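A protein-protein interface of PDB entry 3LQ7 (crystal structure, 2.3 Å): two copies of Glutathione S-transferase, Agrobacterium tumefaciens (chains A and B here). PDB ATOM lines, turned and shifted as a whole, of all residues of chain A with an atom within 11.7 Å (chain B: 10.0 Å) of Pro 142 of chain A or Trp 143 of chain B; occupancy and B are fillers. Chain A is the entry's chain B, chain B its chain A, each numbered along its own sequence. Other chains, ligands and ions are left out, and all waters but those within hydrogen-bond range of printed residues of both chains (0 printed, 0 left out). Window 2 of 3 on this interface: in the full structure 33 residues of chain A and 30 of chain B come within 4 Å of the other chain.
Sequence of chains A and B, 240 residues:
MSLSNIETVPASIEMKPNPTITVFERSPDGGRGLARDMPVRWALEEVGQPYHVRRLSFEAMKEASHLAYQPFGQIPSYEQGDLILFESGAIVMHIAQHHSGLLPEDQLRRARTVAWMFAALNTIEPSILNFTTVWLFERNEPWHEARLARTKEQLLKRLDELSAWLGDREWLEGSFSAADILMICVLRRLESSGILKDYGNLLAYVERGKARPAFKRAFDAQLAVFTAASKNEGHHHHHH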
ATOM      1  N   THR A 133     -22.422  -8.913 -17.041  1.00  0.00           N
ATOM      2  CA  THR A 133     -22.248  -9.612 -18.318  1.00  0.00           C
ATOM      3  C   THR A 133     -23.556 -10.208 -18.853  1.00  0.00           C
ATOM      4  O   THR A 133     -23.691 -10.431 -20.057  1.00  0.00           O
ATOM      5  CB  THR A 133     -21.148 -10.697 -18.260  1.00  0.00           C
ATOM      6  OG1 THR A 133     -21.260 -11.432 -17.035  1.00  0.00           O
ATOM      7  CG2 THR A 133     -19.759 -10.068 -18.357  1.00  0.00           C
ATOM      8  N   VAL A 134     -24.510 -10.466 -17.959  1.00  0.00           N
ATOM      9  CA  VAL A 134     -25.856 -10.870 -18.370  1.00  0.00           C
ATOM     10  C   VAL A 134     -26.667  -9.623 -18.739  1.00  0.00           C
ATOM     11  O   VAL A 134     -27.266  -9.561 -19.817  1.00  0.00           O
ATOM     12  CB  VAL A 134     -26.586 -11.694 -17.273  1.00  0.00           C
ATOM     13  CG1 VAL A 134     -27.958 -12.137 -17.753  1.00  0.00           C
ATOM     14  CG2 VAL A 134     -25.769 -12.905 -16.885  1.00  0.00           C
ATOM     15  N   PHE A 137     -24.135  -7.773 -21.955  1.00  0.00           N
ATOM     16  CA  PHE A 137     -23.562  -8.530 -23.077  1.00  0.00           C
ATOM     17  C   PHE A 137     -24.417  -9.682 -23.626  1.00  0.00           C
ATOM     18  O   PHE A 137     -24.246 -10.086 -24.779  1.00  0.00           O
ATOM     19  CB  PHE A 137     -22.163  -9.047 -22.717  1.00  0.00           C
ATOM     20  CG  PHE A 137     -21.086  -8.006 -22.816  1.00  0.00           C
ATOM     21  CD1 PHE A 137     -20.356  -7.852 -23.994  1.00  0.00           C
ATOM     22  CD2 PHE A 137     -20.793  -7.179 -21.734  1.00  0.00           C
ATOM     23  CE1 PHE A 137     -19.352  -6.889 -24.094  1.00  0.00           C
ATOM     24  CE2 PHE A 137     -19.792  -6.212 -21.824  1.00  0.00           C
ATOM     25  CZ  PHE A 137     -19.070  -6.068 -23.006  1.00  0.00           C
ATOM     26  N   GLU A 138     -25.325 -10.208 -22.806  1.00  0.00           N
ATOM     27  CA  GLU A 138     -26.132 -11.366 -23.204  1.00  0.00           C
ATOM     28  C   GLU A 138     -27.640 -11.090 -23.175  1.00  0.00           C
ATOM     29  O   GLU A 138     -28.411 -11.818 -22.545  1.00  0.00           O
ATOM     30  CB  GLU A 138     -25.769 -12.596 -22.360  1.00  0.00           C
ATOM     31  CG  GLU A 138     -24.403 -13.203 -22.695  1.00  0.00           C
ATOM     32  CD  GLU A 138     -23.991 -14.320 -21.751  1.00  0.00           C
ATOM     33  OE1 GLU A 138     -24.296 -14.242 -20.539  1.00  0.00           O
ATOM     34  OE2 GLU A 138     -23.347 -15.281 -22.221  1.00  0.00           O
ATOM     35  N   ARG A 139     -28.046 -10.032 -23.873  1.00  0.00           N
ATOM     36  CA  ARG A 139     -29.458  -9.686 -24.039  1.00  0.00           C
ATOM     37  C   ARG A 139     -30.134 -10.602 -25.062  1.00  0.00           C
ATOM     38  O   ARG A 139     -31.255 -11.067 -24.847  1.00  0.00           O
ATOM     39  CB  ARG A 139     -29.605  -8.222 -24.477  1.00  0.00           C
ATOM     40  CG  ARG A 139     -29.297  -7.184 -23.399  1.00  0.00           C
ATOM     41  CD  ARG A 139     -30.507  -6.912 -22.516  1.00  0.00           C
ATOM     42  NE  ARG A 139     -30.226  -5.901 -21.499  1.00  0.00           N
ATOM     43  CZ  ARG A 139     -31.042  -5.587 -20.495  1.00  0.00           C
ATOM     44  NH1 ARG A 139     -32.208  -6.204 -20.349  1.00  0.00           N
ATOM     45  NH2 ARG A 139     -30.687  -4.650 -19.625  1.00  0.00           N
ATOM     46  N   ASN A 140     -29.432 -10.862 -26.166  1.00  0.00           N
ATOM     47  CA  ASN A 140     -29.968 -11.621 -27.301  1.00  0.00           C
ATOM     48  C   ASN A 140     -30.015 -13.136 -27.108  1.00  0.00           C
ATOM     49  O   ASN A 140     -30.629 -13.850 -27.905  1.00  0.00           O
ATOM     50  CB  ASN A 140     -29.187 -11.286 -28.576  1.00  0.00           C
ATOM     51  CG  ASN A 140     -29.421  -9.866 -29.051  1.00  0.00           C
ATOM     52  OD1 ASN A 140     -28.472  -9.126 -29.311  1.00  0.00           O
ATOM     53  ND2 ASN A 140     -30.687  -9.475 -29.167  1.00  0.00           N
ATOM     54  N   GLU A 141     -29.357 -13.621 -26.058  1.00  0.00           N
ATOM     55  CA  GLU A 141     -29.368 -15.041 -25.725  1.00  0.00           C
ATOM     56  C   GLU A 141     -30.709 -15.398 -25.075  1.00  0.00           C
ATOM     57  O   GLU A 141     -31.187 -14.659 -24.210  1.00  0.00           O
ATOM     58  CB  GLU A 141     -28.194 -15.387 -24.800  1.00  0.00           C
ATOM     59  CG  GLU A 141     -26.830 -14.844 -25.248  1.00  0.00           C
ATOM     60  CD  GLU A 141     -26.484 -15.177 -26.697  1.00  0.00           C
ATOM     61  OE1 GLU A 141     -26.214 -14.235 -27.472  1.00  0.00           O
ATOM     62  OE2 GLU A 141     -26.486 -16.373 -27.060  1.00  0.00           O
ATOM     63  N   PRO A 142     -31.324 -16.527 -25.494  1.00  0.00           N
ATOM     64  CA  PRO A 142     -32.683 -16.900 -25.061  1.00  0.00           C
ATOM     65  C   PRO A 142     -32.831 -17.335 -23.594  1.00  0.00           C
ATOM     66  O   PRO A 142     -33.949 -17.613 -23.150  1.00  0.00           O
ATOM     67  CB  PRO A 142     -33.041 -18.059 -25.999  1.00  0.00           C
ATOM     68  CG  PRO A 142     -31.734 -18.644 -26.385  1.00  0.00           C
ATOM     69  CD  PRO A 142     -30.784 -17.490 -26.474  1.00  0.00           C
ATOM     70  N   TRP A 143     -31.724 -17.386 -22.855  1.00  0.00           N
ATOM     71  CA  TRP A 143     -31.750 -17.731 -21.432  1.00  0.00           C
ATOM     72  C   TRP A 143     -31.642 -16.503 -20.510  1.00  0.00           C
ATOM     73  O   TRP A 143     -31.242 -16.627 -19.349  1.00  0.00           O
ATOM     74  CB  TRP A 143     -30.655 -18.762 -21.108  1.00  0.00           C
ATOM     75  CG  TRP A 143     -29.227 -18.297 -21.333  1.00  0.00           C
ATOM     76  CD1 TRP A 143     -28.441 -17.600 -20.456  1.00  0.00           C
ATOM     77  CD2 TRP A 143     -28.415 -18.528 -22.496  1.00  0.00           C
ATOM     78  NE1 TRP A 143     -27.204 -17.369 -21.004  1.00  0.00           N
ATOM     79  CE2 TRP A 143     -27.157 -17.928 -22.253  1.00  0.00           C
ATOM     80  CE3 TRP A 143     -28.631 -19.177 -23.721  1.00  0.00           C
ATOM     81  CZ2 TRP A 143     -26.116 -17.959 -23.189  1.00  0.00           C
ATOM     82  CZ3 TRP A 143     -27.593 -19.207 -24.654  1.00  0.00           C
ATOM     83  CH2 TRP A 143     -26.352 -18.600 -24.379  1.00  0.00           C
ATOM     84  N   HIS A 144     -32.035 -15.338 -21.028  1.00  0.00           N
ATOM     85  CA  HIS A 144     -31.783 -14.044 -20.375  1.00  0.00           C
ATOM     86  C   HIS A 144     -32.418 -13.856 -18.992  1.00  0.00           C
ATOM     87  O   HIS A 144     -31.693 -13.743 -18.005  1.00  0.00           O
ATOM     88  CB  HIS A 144     -32.158 -12.876 -21.297  1.00  0.00           C
ATOM     89  CG  HIS A 144     -31.758 -11.535 -20.761  1.00  0.00           C
ATOM     90  ND1 HIS A 144     -30.500 -11.005 -20.952  1.00  0.00           N
ATOM     91  CD2 HIS A 144     -32.444 -10.624 -20.031  1.00  0.00           C
ATOM     92  CE1 HIS A 144     -30.429  -9.823 -20.365  1.00  0.00           C
ATOM     93  NE2 HIS A 144     -31.594  -9.569 -19.798  1.00  0.00           N
ATOM     94  N   GLU A 145     -33.750 -13.827 -18.927  1.00  0.00           N
ATOM     95  CA  GLU A 145     -34.481 -13.512 -17.685  1.00  0.00           C
ATOM     96  C   GLU A 145     -34.321 -14.543 -16.563  1.00  0.00           C
ATOM     97  O   GLU A 145     -34.528 -14.223 -15.389  1.00  0.00           O
ATOM     98  CB  GLU A 145     -35.971 -13.233 -17.950  1.00  0.00           C
ATOM     99  CG  GLU A 145     -36.667 -14.200 -18.906  1.00  0.00           C
ATOM    100  CD  GLU A 145     -36.684 -13.699 -20.344  1.00  0.00           C
ATOM    101  OE1 GLU A 145     -36.351 -14.490 -21.252  1.00  0.00           O
ATOM    102  OE2 GLU A 145     -37.030 -12.518 -20.568  1.00  0.00           O
ATOM    103  N   ALA A 146     -33.955 -15.768 -16.931  1.00  0.00           N
ATOM    104  CA  ALA A 146     -33.634 -16.808 -15.961  1.00  0.00           C
ATOM    105  C   ALA A 146     -32.279 -16.535 -15.299  1.00  0.00           C
ATOM    106  O   ALA A 146     -32.155 -16.577 -14.070  1.00  0.00           O
ATOM    107  CB  ALA A 146     -33.641 -18.178 -16.633  1.00  0.00           C
ATOM    108  N   ARG A 147     -31.279 -16.238 -16.127  1.00  0.00           N
ATOM    109  CA  ARG A 147     -29.902 -16.021 -15.681  1.00  0.00           C
ATOM    110  C   ARG A 147     -29.725 -14.679 -14.954  1.00  0.00           C
ATOM    111  O   ARG A 147     -28.979 -14.591 -13.973  1.00  0.00           O
ATOM    112  CB  ARG A 147     -28.949 -16.132 -16.882  1.00  0.00           C
ATOM    113  CG  ARG A 147     -27.470 -16.208 -16.536  1.00  0.00           C
ATOM    114  CD  ARG A 147     -27.095 -17.512 -15.844  1.00  0.00           C
ATOM    115  NE  ARG A 147     -26.142 -17.281 -14.757  1.00  0.00           N
ATOM    116  CZ  ARG A 147     -24.819 -17.238 -14.897  1.00  0.00           C
ATOM    117  NH1 ARG A 147     -24.256 -17.420 -16.088  1.00  0.00           N
ATOM    118  NH2 ARG A 147     -24.053 -17.018 -13.834  1.00  0.00           N
ATOM    119  N   LEU A 148     -30.422 -13.652 -15.443  1.00  0.00           N
ATOM    120  CA  LEU A 148     -30.397 -12.303 -14.868  1.00  0.00           C
ATOM    121  C   LEU A 148     -30.902 -12.270 -13.430  1.00  0.00           C
ATOM    122  O   LEU A 148     -30.324 -11.585 -12.589  1.00  0.00           O
ATOM    123  CB  LEU A 148     -31.218 -11.338 -15.739  1.00  0.00           C
ATOM    124  CG  LEU A 148     -31.290  -9.837 -15.427  1.00  0.00           C
ATOM    125  CD1 LEU A 148     -29.987  -9.119 -15.777  1.00  0.00           C
ATOM    126  CD2 LEU A 148     -32.475  -9.196 -16.153  1.00  0.00           C
ATOM    127  N   ALA A 149     -31.966 -13.021 -13.156  1.00  0.00           N
ATOM    128  CA  ALA A 149     -32.574 -13.068 -11.828  1.00  0.00           C
ATOM    129  C   ALA A 149     -31.704 -13.806 -10.809  1.00  0.00           C
ATOM    130  O   ALA A 149     -31.712 -13.468  -9.621  1.00  0.00           O
ATOM    131  CB  ALA A 149     -33.962 -13.696 -11.902  1.00  0.00           C
ATOM    132  N   VAL B 134     -21.849 -24.822 -13.440  1.00  0.00           N
ATOM    133  CA  VAL B 134     -22.696 -25.294 -14.527  1.00  0.00           C
ATOM    134  C   VAL B 134     -22.510 -26.798 -14.691  1.00  0.00           C
ATOM    135  O   VAL B 134     -23.487 -27.547 -14.756  1.00  0.00           O
ATOM    136  CB  VAL B 134     -22.391 -24.544 -15.856  1.00  0.00           C
ATOM    137  CG1 VAL B 134     -23.291 -25.036 -16.985  1.00  0.00           C
ATOM    138  CG2 VAL B 134     -22.584 -23.047 -15.671  1.00  0.00           C
ATOM    139  N   GLU B 138     -25.764 -27.539 -12.518  1.00  0.00           N
ATOM    140  CA  GLU B 138     -26.789 -26.932 -13.370  1.00  0.00           C
ATOM    141  C   GLU B 138     -27.241 -27.818 -14.539  1.00  0.00           C
ATOM    142  O   GLU B 138     -27.480 -27.334 -15.650  1.00  0.00           O
ATOM    143  CB  GLU B 138     -26.359 -25.531 -13.824  1.00  0.00           C
ATOM    144  CG  GLU B 138     -26.188 -24.547 -12.661  1.00  0.00           C
ATOM    145  CD  GLU B 138     -26.197 -23.087 -13.084  1.00  0.00           C
ATOM    146  OE1 GLU B 138     -25.522 -22.731 -14.076  1.00  0.00           O
ATOM    147  OE2 GLU B 138     -26.872 -22.288 -12.402  1.00  0.00           O
ATOM    148  N   ARG B 139     -27.384 -29.113 -14.257  1.00  0.00           N
ATOM    149  CA  ARG B 139     -27.914 -30.087 -15.217  1.00  0.00           C
ATOM    150  C   ARG B 139     -29.446 -30.000 -15.300  1.00  0.00           C
ATOM    151  O   ARG B 139     -30.062 -30.550 -16.217  1.00  0.00           O
ATOM    152  CB  ARG B 139     -27.471 -31.510 -14.838  1.00  0.00           C
ATOM    153  CG  ARG B 139     -25.953 -31.705 -14.710  1.00  0.00           C
ATOM    154  CD  ARG B 139     -25.306 -32.124 -16.031  1.00  0.00           C
ATOM    155  NE  ARG B 139     -23.880 -31.789 -16.094  1.00  0.00           N
ATOM    156  CZ  ARG B 139     -23.044 -32.203 -17.048  1.00  0.00           C
ATOM    157  NH1 ARG B 139     -23.477 -32.980 -18.033  1.00  0.00           N
ATOM    158  NH2 ARG B 139     -21.768 -31.843 -17.016  1.00  0.00           N
ATOM    159  N   ASN B 140     -30.039 -29.301 -14.332  1.00  0.00           N
ATOM    160  CA  ASN B 140     -31.481 -29.051 -14.260  1.00  0.00           C
ATOM    161  C   ASN B 140     -31.948 -27.906 -15.176  1.00  0.00           C
ATOM    162  O   ASN B 140     -33.112 -27.856 -15.578  1.00  0.00           O
ATOM    163  CB  ASN B 140     -31.863 -28.759 -12.800  1.00  0.00           C
ATOM    164  CG  ASN B 140     -33.366 -28.650 -12.581  1.00  0.00           C
ATOM    165  OD1 ASN B 140     -33.832 -27.772 -11.852  1.00  0.00           O
ATOM    166  ND2 ASN B 140     -34.130 -29.541 -13.208  1.00  0.00           N
ATOM    167  N   GLU B 141     -31.026 -27.001 -15.505  1.00  0.00           N
ATOM    168  CA  GLU B 141     -31.330 -25.785 -16.267  1.00  0.00           C
ATOM    169  C   GLU B 141     -31.622 -26.073 -17.747  1.00  0.00           C
ATOM    170  O   GLU B 141     -31.042 -27.002 -18.312  1.00  0.00           O
ATOM    171  CB  GLU B 141     -30.182 -24.778 -16.123  1.00  0.00           C
ATOM    172  CG  GLU B 141     -29.782 -24.474 -14.680  1.00  0.00           C
ATOM    173  CD  GLU B 141     -30.962 -24.155 -13.785  1.00  0.00           C
ATOM    174  OE1 GLU B 141     -31.247 -24.965 -12.877  1.00  0.00           O
ATOM    175  OE2 GLU B 141     -31.605 -23.104 -13.998  1.00  0.00           O
ATOM    176  N   PRO B 142     -32.531 -25.284 -18.371  1.00  0.00           N
ATOM    177  CA  PRO B 142     -33.003 -25.544 -19.743  1.00  0.00           C
ATOM    178  C   PRO B 142     -31.958 -25.403 -20.858  1.00  0.00           C
ATOM    179  O   PRO B 142     -31.904 -26.258 -21.750  1.00  0.00           O
ATOM    180  CB  PRO B 142     -34.129 -24.518 -19.933  1.00  0.00           C
ATOM    181  CG  PRO B 142     -33.867 -23.462 -18.925  1.00  0.00           C
ATOM    182  CD  PRO B 142     -33.278 -24.171 -17.753  1.00  0.00           C
ATOM    183  N   TRP B 143     -31.148 -24.345 -20.806  1.00  0.00           N
ATOM    184  CA  TRP B 143     -30.109 -24.096 -21.813  1.00  0.00           C
ATOM    185  C   TRP B 143     -28.723 -24.459 -21.281  1.00  0.00           C
ATOM    186  O   TRP B 143     -27.723 -23.812 -21.617  1.00  0.00           O
ATOM    187  CB  TRP B 143     -30.143 -22.637 -22.269  1.00  0.00           C
ATOM    188  CG  TRP B 143     -31.400 -22.264 -22.993  1.00  0.00           C
ATOM    189  CD1 TRP B 143     -32.530 -21.721 -22.448  1.00  0.00           C
ATOM    190  CD2 TRP B 143     -31.656 -22.403 -24.396  1.00  0.00           C
ATOM    191  NE1 TRP B 143     -33.474 -21.512 -23.427  1.00  0.00           N
ATOM    192  CE2 TRP B 143     -32.965 -21.923 -24.631  1.00  0.00           C
ATOM    193  CE3 TRP B 143     -30.907 -22.888 -25.479  1.00  0.00           C
ATOM    194  CZ2 TRP B 143     -33.541 -21.908 -25.908  1.00  0.00           C
ATOM    195  CZ3 TRP B 143     -31.482 -22.876 -26.750  1.00  0.00           C
ATOM    196  CH2 TRP B 143     -32.788 -22.388 -26.951  1.00  0.00           C
ATOM    197  N   HIS B 144     -28.700 -25.509 -20.456  1.00  0.00           N
ATOM    198  CA  HIS B 144     -27.505 -26.057 -19.806  1.00  0.00           C
ATOM    199  C   HIS B 144     -26.338 -26.294 -20.762  1.00  0.00           C
ATOM    200  O   HIS B 144     -25.206 -25.919 -20.463  1.00  0.00           O
ATOM    201  CB  HIS B 144     -27.880 -27.363 -19.080  1.00  0.00           C
ATOM    202  CG  HIS B 144     -26.707 -28.204 -18.691  1.00  0.00           C
ATOM    203  ND1 HIS B 144     -25.912 -27.915 -17.603  1.00  0.00           N
ATOM    204  CD2 HIS B 144     -26.198 -29.332 -19.240  1.00  0.00           C
ATOM    205  CE1 HIS B 144     -24.960 -28.826 -17.502  1.00  0.00           C
ATOM    206  NE2 HIS B 144     -25.110 -29.695 -18.485  1.00  0.00           N
ATOM    207  N   GLU B 145     -26.639 -26.912 -21.903  1.00  0.00           N
ATOM    208  CA  GLU B 145     -25.665 -27.237 -22.947  1.00  0.00           C
ATOM    209  C   GLU B 145     -24.907 -26.021 -23.492  1.00  0.00           C
ATOM    210  O   GLU B 145     -23.681 -26.059 -23.618  1.00  0.00           O
ATOM    211  CB  GLU B 145     -26.346 -27.998 -24.101  1.00  0.00           C
ATOM    212  CG  GLU B 145     -27.775 -27.513 -24.463  1.00  0.00           C
ATOM    213  CD  GLU B 145     -28.871 -28.346 -23.811  1.00  0.00           C
ATOM    214  OE1 GLU B 145     -29.602 -27.821 -22.936  1.00  0.00           O
ATOM    215  OE2 GLU B 145     -28.999 -29.535 -24.173  1.00  0.00           O
ATOM    216  N   ALA B 146     -25.642 -24.950 -23.789  1.00  0.00           N
ATOM    217  CA  ALA B 146     -25.083 -23.760 -24.435  1.00  0.00           C
ATOM    218  C   ALA B 146     -24.277 -22.883 -23.474  1.00  0.00           C
ATOM    219  O   ALA B 146     -23.281 -22.269 -23.870  1.00  0.00           O
ATOM    220  CB  ALA B 146     -26.191 -22.951 -25.093  1.00  0.00           C
ATOM    221  N   ARG B 147     -24.715 -22.832 -22.219  1.00  0.00           N
ATOM    222  CA  ARG B 147     -24.040 -22.049 -21.187  1.00  0.00           C
ATOM    223  C   ARG B 147     -22.736 -22.724 -20.747  1.00  0.00           C
ATOM    224  O   ARG B 147     -21.748 -22.044 -20.450  1.00  0.00           O
ATOM    225  CB  ARG B 147     -24.972 -21.833 -19.995  1.00  0.00           C
ATOM    226  CG  ARG B 147     -24.555 -20.699 -19.057  1.00  0.00           C
ATOM    227  CD  ARG B 147     -25.633 -20.372 -18.024  1.00  0.00           C
ATOM    228  NE  ARG B 147     -25.894 -21.489 -17.115  1.00  0.00           N
ATOM    229  CZ  ARG B 147     -26.957 -22.286 -17.175  1.00  0.00           C
ATOM    230  NH1 ARG B 147     -27.890 -22.108 -18.103  1.00  0.00           N
ATOM    231  NH2 ARG B 147     -27.085 -23.272 -16.304  1.00  0.00           N
ATOM    232  N   LEU B 148     -22.750 -24.058 -20.725  1.00  0.00           N
ATOM    233  CA  LEU B 148     -21.578 -24.865 -20.398  1.00  0.00           C
ATOM    234  C   LEU B 148     -20.457 -24.637 -21.405  1.00  0.00           C
ATOM    235  O   LEU B 148     -19.292 -24.520 -21.022  1.00  0.00           O
ATOM    236  CB  LEU B 148     -21.948 -26.353 -20.349  1.00  0.00           C
ATOM    237  CG  LEU B 148     -20.894 -27.403 -19.979  1.00  0.00           C
ATOM    238  CD1 LEU B 148     -20.645 -27.410 -18.491  1.00  0.00           C
ATOM    239  CD2 LEU B 148     -21.330 -28.779 -20.449  1.00  0.00           C
ATOM    240  N   ALA B 149     -20.829 -24.560 -22.683  1.00  0.00           N
ATOM    241  CA  ALA B 149     -19.889 -24.341 -23.782  1.00  0.00           C
ATOM    242  C   ALA B 149     -19.242 -22.960 -23.722  1.00  0.00           C
ATOM    243  O   ALA B 149     -18.081 -22.799 -24.112  1.00  0.00           O
ATOM    244  CB  ALA B 149     -20.588 -24.546 -25.133  1.00  0.00           C
ATOM    245  N   ARG B 150     -19.994 -21.978 -23.226  1.00  0.00           N
ATOM    246  CA  ARG B 150     -19.511 -20.600 -23.149  1.00  0.00           C
ATOM    247  C   ARG B 150     -18.505 -20.436 -22.007  1.00  0.00           C
ATOM    248  O   ARG B 150     -17.475 -19.767 -22.167  1.00  0.00           O
ATOM    249  CB  ARG B 150     -20.674 -19.608 -23.001  1.00  0.00           C
ATOM    250  CG  ARG B 150     -20.515 -18.324 -23.821  1.00  0.00           C
ATOM    251  CD  ARG B 150     -19.639 -17.279 -23.128  1.00  0.00           C
ATOM    252  NE  ARG B 150     -18.963 -16.397 -24.081  1.00  0.00           N
ATOM    253  CZ  ARG B 150     -19.458 -15.246 -24.539  1.00  0.00           C
ATOM    254  NH1 ARG B 150     -20.649 -14.815 -24.138  1.00  0.00           N
ATOM    255  NH2 ARG B 150     -18.757 -14.523 -25.403  1.00  0.00           N
ATOM    256  N   THR B 151     -18.801 -21.052 -20.866  1.00  0.00           N
ATOM    257  CA  THR B 151     -17.906 -20.965 -19.713  1.00  0.00           C
ATOM    258  C   THR B 151     -16.639 -21.803 -19.900  1.00  0.00           C
ATOM    259  O   THR B 151     -15.566 -21.399 -19.453  1.00  0.00           O
ATOM    260  CB  THR B 151     -18.615 -21.310 -18.400  1.00  0.00           C
ATOM    261  OG1 THR B 151     -19.067 -22.667 -18.435  1.00  0.00           O
ATOM    262  CG2 THR B 151     -19.801 -20.371 -18.172  1.00  0.00           C
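The side-chain carboxylate of Glu 138 of chain A is in salt-bridge range of the guanidinium group of Arg 150 of chain B (3.3 Å).
The backbone carbonyl oxygen of Thr 133 of chain A is in hydrogen-bond range of the backbone NH of Glu 138 of chain A (3.2 Å).
The backbone carbonyl oxygen of Arg 147 of chain B sits at hydrogen-bond distance from the side-chain hydroxyl of Thr 151 of chain B (3.4 Å).
OE1 of Glu 138 of chain B lies within salt-bridge range of NH2 of Arg 147 of chain B (2.8 Å).
The backbone carbonyl oxygen (O) of Glu 138 of chain A is in hydrogen-bond range of a ring nitrogen (ND1) of His 144 of chain A (2.8 Å).
Among the printed residues, pairs that only touch across the chains: Pro 142 of chain A with Trp 143 of chain B, Trp 143 of chain A with Trp 143 of chain B and Arg 147 of chain A with Arg 147 of chain B.
Printed residues of chain B within 4 Å of Glu 138 of chain A: Arg 150 (3.3 Å).
Of chain B, only Trp 143 comes within 4 Å of Pro 142 of chain A.
Of the printed residues of chain B, Trp 143 of chain A touches Trp 143.
Printed residues of chain B within 4 Å of Arg 147 of chain A: Arg 147.
Asn 140 of chain B touches none of the printed residues of chain A.
No residue of chain A comes within 4 Å of Pro 142 of chain B.
Trp 143 of chain B touches just these residues of chain A: Pro 142 and Trp 143.
No residue of chain A comes within 4 Å of His 144 of chain B.
No residue of chain A comes within 4 Å of Ala 146 of chain B.
Of chain A, only Arg 147 comes within 4 Å of Arg 147 of chain B.
Of the printed residues of chain A, Arg 150 of chain B touches Glu 138.
The nearest residue of chain B that does not touch Pro 142 of chain A is Ala 146 of chain B (7.1 Å).
The nearest residue of chain A that does not touch Trp 143 of chain B is His 144 of chain A (6.6 Å).
The nearest printed residue of chain B that does not touch Glu 138 of chain A is Arg 147 of chain B (6.4 Å).
Printed residues of chain A that touch a printed residue of chain B: Glu 138, Pro 142, Trp 143 and Arg 147.
Hydrophobic or aromatic side chains of chain A within 4 Å of the printed part of chain B: Pro 142 and Trp 143.
Among the printed residues, 4 pairs touch across the chains.
Pro 142 of chain A touches Trp 143 of chain B, but with the chains exchanged Trp 143 of chain A does not touch Pro 142 of chain B (6.1 Å).
Trp 143 of chain A touches its own counterpart, Trp 143 of chain B.
Arg 147 of chain A touches its own counterpart, Arg 147 of chain B.
Positions printed for both chains: 134, 138, 139, 140, 141, 142, 143, 144, 145, 146, 147, 148 and 149.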
